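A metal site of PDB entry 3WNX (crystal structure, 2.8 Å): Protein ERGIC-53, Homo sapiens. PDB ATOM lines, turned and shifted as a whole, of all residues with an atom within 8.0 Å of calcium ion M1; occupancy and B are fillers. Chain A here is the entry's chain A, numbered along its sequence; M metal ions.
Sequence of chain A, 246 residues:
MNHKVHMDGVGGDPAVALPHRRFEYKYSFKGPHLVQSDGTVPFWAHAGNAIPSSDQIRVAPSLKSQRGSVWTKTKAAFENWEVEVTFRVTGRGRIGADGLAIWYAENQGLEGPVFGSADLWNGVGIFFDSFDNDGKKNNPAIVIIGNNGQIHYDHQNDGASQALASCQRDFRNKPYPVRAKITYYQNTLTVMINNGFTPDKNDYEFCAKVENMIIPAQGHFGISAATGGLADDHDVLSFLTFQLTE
The backbone NH (N) of Lys 137 lies within hydrogen-bond range of the side-chain carboxylate (OD2) of Asp 132, at 2.7 Å.
The side-chain amide nitrogen (NE2) of Gln 168 lies close to the backbone carbonyl oxygen (O) of Asn 138, at 3.3 Å.
The backbone NH (N) of Asp 132 sits close to the side-chain amide nitrogen (ND2) of Asn 139, at 3.1 Å.
The backbone NH of Asp 134 lies within hydrogen-bond range of the backbone carbonyl oxygen of Gln 156 (3.1 Å).
The side-chain amide oxygen (OD1) of Asn 139 lies close to the side-chain amide nitrogen (ND2) of Asn 138, at 3.4 Å.
ND2 of Asn 139 sits close to O of Phe 131, 2.6 Å away.
OD2 of Asp 132 lies within hydrogen-bond range of N of Lys 136 (3.2 Å).
The backbone carbonyl oxygen of Asp 129 lies within hydrogen-bond range of the side-chain amide nitrogen of Asn 139, 3.2 Å away.
Asn 133 touches calcium ion M1 (N to CA, 3.5 Å).
Six residues have an atom within 4 Å of calcium ion M1: Asp 132, Asn 133, Asp 134, Asn 138, Asn 139 and Asp 158.
Along chain A the residues within 4 Å of calcium ion M1 span positions 132 to 158.
Calcium ion M1 is bound by OD2 of Asp 158 (1.9 Å), OD1 of Asn 138 (2.2 Å), OD1 of Asp 132 (2.5 Å) and OD1 of Asp 134 (2.6 Å).
Calcium ion M1 has four donor atoms within binding distance.
Slightly farther from calcium ion M1 lies the side-chain amide oxygen (OD1) of Asn 139 (3.1 Å).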
ATOM      1  N   ASP A 129      19.961  -3.613  -1.306  1.00  0.00           N
ATOM      2  CA  ASP A 129      19.648  -4.538  -2.399  1.00  0.00           C
ATOM      3  C   ASP A 129      20.155  -3.993  -3.717  1.00  0.00           C
ATOM      4  O   ASP A 129      19.540  -3.113  -4.317  1.00  0.00           O
ATOM      5  CB  ASP A 129      18.141  -4.778  -2.463  1.00  0.00           C
ATOM      6  CG  ASP A 129      17.744  -6.003  -3.274  1.00  0.00           C
ATOM      7  OD1 ASP A 129      18.354  -6.275  -4.343  1.00  0.00           O
ATOM      8  OD2 ASP A 129      16.806  -6.718  -2.843  1.00  0.00           O
ATOM      9  N   SER A 130      21.307  -4.508  -4.164  1.00  0.00           N
ATOM     10  CA  SER A 130      21.879  -4.126  -5.453  1.00  0.00           C
ATOM     11  C   SER A 130      20.993  -4.625  -6.588  1.00  0.00           C
ATOM     12  O   SER A 130      20.824  -3.935  -7.592  1.00  0.00           O
ATOM     13  CB  SER A 130      23.283  -4.726  -5.657  1.00  0.00           C
ATOM     14  OG  SER A 130      24.106  -4.590  -4.511  1.00  0.00           O
ATOM     15  N   PHE A 131      20.461  -5.838  -6.419  1.00  0.00           N
ATOM     16  CA  PHE A 131      19.818  -6.527  -7.540  1.00  0.00           C
ATOM     17  C   PHE A 131      18.282  -6.468  -7.550  1.00  0.00           C
ATOM     18  O   PHE A 131      17.588  -6.923  -6.620  1.00  0.00           O
ATOM     19  CB  PHE A 131      20.281  -7.982  -7.627  1.00  0.00           C
ATOM     20  CG  PHE A 131      19.885  -8.639  -8.922  1.00  0.00           C
ATOM     21  CD1 PHE A 131      20.328  -8.131 -10.137  1.00  0.00           C
ATOM     22  CD2 PHE A 131      19.039  -9.756  -8.933  1.00  0.00           C
ATOM     23  CE1 PHE A 131      19.961  -8.728 -11.339  1.00  0.00           C
ATOM     24  CE2 PHE A 131      18.661 -10.359 -10.126  1.00  0.00           C
ATOM     25  CZ  PHE A 131      19.126  -9.846 -11.337  1.00  0.00           C
ATOM     26  N   ASP A 132      17.789  -5.919  -8.663  1.00  0.00           N
ATOM     27  CA  ASP A 132      16.379  -5.727  -8.945  1.00  0.00           C
ATOM     28  C   ASP A 132      15.610  -7.069  -9.105  1.00  0.00           C
ATOM     29  O   ASP A 132      15.219  -7.437 -10.222  1.00  0.00           O
ATOM     30  CB  ASP A 132      16.277  -4.884 -10.229  1.00  0.00           C
ATOM     31  CG  ASP A 132      14.875  -4.430 -10.532  1.00  0.00           C
ATOM     32  OD1 ASP A 132      14.122  -4.135  -9.574  1.00  0.00           O
ATOM     33  OD2 ASP A 132      14.529  -4.345 -11.727  1.00  0.00           O
ATOM     34  N   ASN A 133      15.373  -7.771  -7.999  1.00  0.00           N
ATOM     35  CA  ASN A 133      14.883  -9.161  -8.070  1.00  0.00           C
ATOM     36  C   ASN A 133      13.418  -9.344  -8.512  1.00  0.00           C
ATOM     37  O   ASN A 133      13.082 -10.396  -9.075  1.00  0.00           O
ATOM     38  CB  ASN A 133      15.122  -9.911  -6.758  1.00  0.00           C
ATOM     39  CG  ASN A 133      16.594 -10.154  -6.495  1.00  0.00           C
ATOM     40  OD1 ASN A 133      17.358  -9.211  -6.237  1.00  0.00           O
ATOM     41  ND2 ASN A 133      17.016 -11.416  -6.530  1.00  0.00           N
ATOM     42  N   ASP A 134      12.554  -8.360  -8.252  1.00  0.00           N
ATOM     43  CA  ASP A 134      11.161  -8.404  -8.746  1.00  0.00           C
ATOM     44  C   ASP A 134      11.002  -7.643 -10.076  1.00  0.00           C
ATOM     45  O   ASP A 134       9.903  -7.234 -10.436  1.00  0.00           O
ATOM     46  CB  ASP A 134      10.147  -7.938  -7.685  1.00  0.00           C
ATOM     47  CG  ASP A 134      10.613  -6.721  -6.882  1.00  0.00           C
ATOM     48  OD1 ASP A 134      11.110  -5.761  -7.505  1.00  0.00           O
ATOM     49  OD2 ASP A 134      10.467  -6.719  -5.644  1.00  0.00           O
ATOM     50  N   GLY A 135      12.112  -7.479 -10.801  1.00  0.00           N
ATOM     51  CA  GLY A 135      12.099  -6.868 -12.120  1.00  0.00           C
ATOM     52  C   GLY A 135      11.541  -5.455 -12.190  1.00  0.00           C
ATOM     53  O   GLY A 135      11.288  -4.953 -13.282  1.00  0.00           O
ATOM     54  N   LYS A 136      11.401  -4.797 -11.049  1.00  0.00           N
ATOM     55  CA  LYS A 136      10.659  -3.539 -10.974  1.00  0.00           C
ATOM     56  C   LYS A 136      11.418  -2.238 -11.375  1.00  0.00           C
ATOM     57  O   LYS A 136      10.809  -1.170 -11.351  1.00  0.00           O
ATOM     58  CB  LYS A 136      10.110  -3.373  -9.544  1.00  0.00           C
ATOM     59  CG  LYS A 136       8.974  -4.320  -9.184  1.00  0.00           C
ATOM     60  CD  LYS A 136       7.618  -3.812  -9.666  1.00  0.00           C
ATOM     61  CE  LYS A 136       6.475  -4.775  -9.348  1.00  0.00           C
ATOM     62  NZ  LYS A 136       5.161  -4.264  -9.829  1.00  0.00           N
ATOM     63  N   LYS A 137      12.694  -2.299 -11.753  1.00  0.00           N
ATOM     64  CA  LYS A 137      13.566  -1.093 -11.864  1.00  0.00           C
ATOM     65  C   LYS A 137      13.734  -0.239 -10.564  1.00  0.00           C
ATOM     66  O   LYS A 137      14.209   0.901 -10.622  1.00  0.00           O
ATOM     67  CB  LYS A 137      13.110  -0.150 -12.987  1.00  0.00           C
ATOM     68  CG  LYS A 137      12.830  -0.795 -14.341  1.00  0.00           C
ATOM     69  CD  LYS A 137      12.789   0.282 -15.430  1.00  0.00           C
ATOM     70  CE  LYS A 137      11.652   0.091 -16.434  1.00  0.00           C
ATOM     71  NZ  LYS A 137      11.965  -0.807 -17.578  1.00  0.00           N
ATOM     72  N   ASN A 138      13.369  -0.789  -9.414  1.00  0.00           N
ATOM     73  CA  ASN A 138      13.365  -0.040  -8.166  1.00  0.00           C
ATOM     74  C   ASN A 138      14.698  -0.157  -7.414  1.00  0.00           C
ATOM     75  O   ASN A 138      14.828   0.265  -6.245  1.00  0.00           O
ATOM     76  CB  ASN A 138      12.236  -0.546  -7.251  1.00  0.00           C
ATOM     77  CG  ASN A 138      12.432  -1.998  -6.862  1.00  0.00           C
ATOM     78  OD1 ASN A 138      12.779  -2.839  -7.699  1.00  0.00           O
ATOM     79  ND2 ASN A 138      12.232  -2.316  -5.587  1.00  0.00           N
ATOM     80  N   ASN A 139      15.683  -0.759  -8.072  1.00  0.00           N
ATOM     81  CA  ASN A 139      16.973  -1.010  -7.465  1.00  0.00           C
ATOM     82  C   ASN A 139      18.066  -0.153  -8.094  1.00  0.00           C
ATOM     83  O   ASN A 139      17.848   0.380  -9.184  1.00  0.00           O
ATOM     84  CB  ASN A 139      17.282  -2.510  -7.524  1.00  0.00           C
ATOM     85  CG  ASN A 139      16.559  -3.273  -6.440  1.00  0.00           C
ATOM     86  OD1 ASN A 139      15.524  -2.840  -5.946  1.00  0.00           O
ATOM     87  ND2 ASN A 139      17.112  -4.393  -6.027  1.00  0.00           N
ATOM     88  N   PRO A 140      19.199   0.048  -7.389  1.00  0.00           N
ATOM     89  CA  PRO A 140      19.477  -0.426  -6.031  1.00  0.00           C
ATOM     90  C   PRO A 140      18.759   0.426  -5.005  1.00  0.00           C
ATOM     91  O   PRO A 140      18.463   1.598  -5.267  1.00  0.00           O
ATOM     92  CB  PRO A 140      21.006  -0.254  -5.882  1.00  0.00           C
ATOM     93  CG  PRO A 140      21.480   0.500  -7.091  1.00  0.00           C
ATOM     94  CD  PRO A 140      20.272   0.930  -7.873  1.00  0.00           C
ATOM     95  N   ALA A 141      18.501  -0.171  -3.845  1.00  0.00           N
ATOM     96  CA  ALA A 141      17.663   0.471  -2.844  1.00  0.00           C
ATOM     97  C   ALA A 141      17.984  -0.026  -1.440  1.00  0.00           C
ATOM     98  O   ALA A 141      18.437  -1.157  -1.263  1.00  0.00           O
ATOM     99  CB  ALA A 141      16.203   0.203  -3.161  1.00  0.00           C
ATOM    100  N   HIS A 155      12.873 -12.892  -0.837  1.00  0.00           N
ATOM    101  CA  HIS A 155      14.077 -12.578  -1.603  1.00  0.00           C
ATOM    102  C   HIS A 155      13.733 -12.100  -3.010  1.00  0.00           C
ATOM    103  O   HIS A 155      14.142 -11.009  -3.407  1.00  0.00           O
ATOM    104  CB  HIS A 155      15.029 -13.781  -1.671  1.00  0.00           C
ATOM    105  CG  HIS A 155      16.370 -13.448  -2.247  1.00  0.00           C
ATOM    106  ND1 HIS A 155      17.492 -13.241  -1.471  1.00  0.00           N
ATOM    107  CD2 HIS A 155      16.773 -13.289  -3.533  1.00  0.00           C
ATOM    108  CE1 HIS A 155      18.527 -12.972  -2.248  1.00  0.00           C
ATOM    109  NE2 HIS A 155      18.120 -12.991  -3.509  1.00  0.00           N
ATOM    110  N   GLN A 156      12.961 -12.913  -3.729  1.00  0.00           N
ATOM    111  CA  GLN A 156      12.642 -12.644  -5.137  1.00  0.00           C
ATOM    112  C   GLN A 156      11.887 -11.337  -5.312  1.00  0.00           C
ATOM    113  O   GLN A 156      11.974 -10.729  -6.380  1.00  0.00           O
ATOM    114  CB  GLN A 156      11.841 -13.784  -5.773  1.00  0.00           C
ATOM    115  CG  GLN A 156      12.611 -15.090  -5.984  1.00  0.00           C
ATOM    116  CD  GLN A 156      12.340 -16.139  -4.907  1.00  0.00           C
ATOM    117  OE1 GLN A 156      12.039 -15.819  -3.758  1.00  0.00           O
ATOM    118  NE2 GLN A 156      12.454 -17.417  -5.288  1.00  0.00           N
ATOM    119  N   ASN A 157      11.159 -10.905  -4.286  1.00  0.00           N
ATOM    120  CA  ASN A 157      10.437  -9.620  -4.322  1.00  0.00           C
ATOM    121  C   ASN A 157      11.114  -8.506  -3.519  1.00  0.00           C
ATOM    122  O   ASN A 157      10.438  -7.580  -3.059  1.00  0.00           O
ATOM    123  CB  ASN A 157       8.991  -9.791  -3.854  1.00  0.00           C
ATOM    124  CG  ASN A 157       8.158 -10.606  -4.830  1.00  0.00           C
ATOM    125  OD1 ASN A 157       8.140 -10.316  -6.034  1.00  0.00           O
ATOM    126  ND2 ASN A 157       7.457 -11.622  -4.322  1.00  0.00           N
ATOM    127  N   ASP A 158      12.431  -8.594  -3.359  1.00  0.00           N
ATOM    128  CA  ASP A 158      13.179  -7.651  -2.550  1.00  0.00           C
ATOM    129  C   ASP A 158      12.598  -7.469  -1.145  1.00  0.00           C
ATOM    130  O   ASP A 158      13.073  -6.621  -0.404  1.00  0.00           O
ATOM    131  CB  ASP A 158      13.224  -6.273  -3.222  1.00  0.00           C
ATOM    132  CG  ASP A 158      13.696  -6.324  -4.656  1.00  0.00           C
ATOM    133  OD1 ASP A 158      14.284  -7.336  -5.073  1.00  0.00           O
ATOM    134  OD2 ASP A 158      13.468  -5.323  -5.368  1.00  0.00           O
ATOM    135  N   GLY A 159      11.574  -8.243  -0.779  1.00  0.00           N
ATOM    136  CA  GLY A 159      10.758  -7.928   0.386  1.00  0.00           C
ATOM    137  C   GLY A 159       9.976  -6.603   0.319  1.00  0.00           C
ATOM    138  O   GLY A 159       9.621  -6.041   1.364  1.00  0.00           O
ATOM    139  N   ALA A 160       9.697  -6.120  -0.896  1.00  0.00           N
ATOM    140  CA  ALA A 160       8.956  -4.863  -1.064  1.00  0.00           C
ATOM    141  C   ALA A 160       7.650  -4.813  -0.240  1.00  0.00           C
ATOM    142  O   ALA A 160       7.194  -3.727   0.107  1.00  0.00           O
ATOM    143  CB  ALA A 160       8.655  -4.630  -2.543  1.00  0.00           C
ATOM    144  N   GLN A 168      15.601   4.778  -2.466  1.00  0.00           N
ATOM    145  CA  GLN A 168      16.281   4.396  -3.689  1.00  0.00           C
ATOM    146  C   GLN A 168      17.549   5.202  -3.908  1.00  0.00           C
ATOM    147  O   GLN A 168      17.570   6.162  -4.700  1.00  0.00           O
ATOM    148  CB  GLN A 168      15.347   4.569  -4.893  1.00  0.00           C
ATOM    149  CG  GLN A 168      14.574   3.315  -5.256  1.00  0.00           C
ATOM    150  CD  GLN A 168      14.309   3.187  -6.750  1.00  0.00           C
ATOM    151  OE1 GLN A 168      13.156   3.042  -7.162  1.00  0.00           O
ATOM    152  NE2 GLN A 168      15.360   3.216  -7.568  1.00  0.00           N
HETATM  153 CA    CA M   1      13.523  -4.849  -7.253  1.00  0.00          CA
HETATM  154 CA    CA M   2      17.253  -8.312  -4.370  1.00  0.00          CA
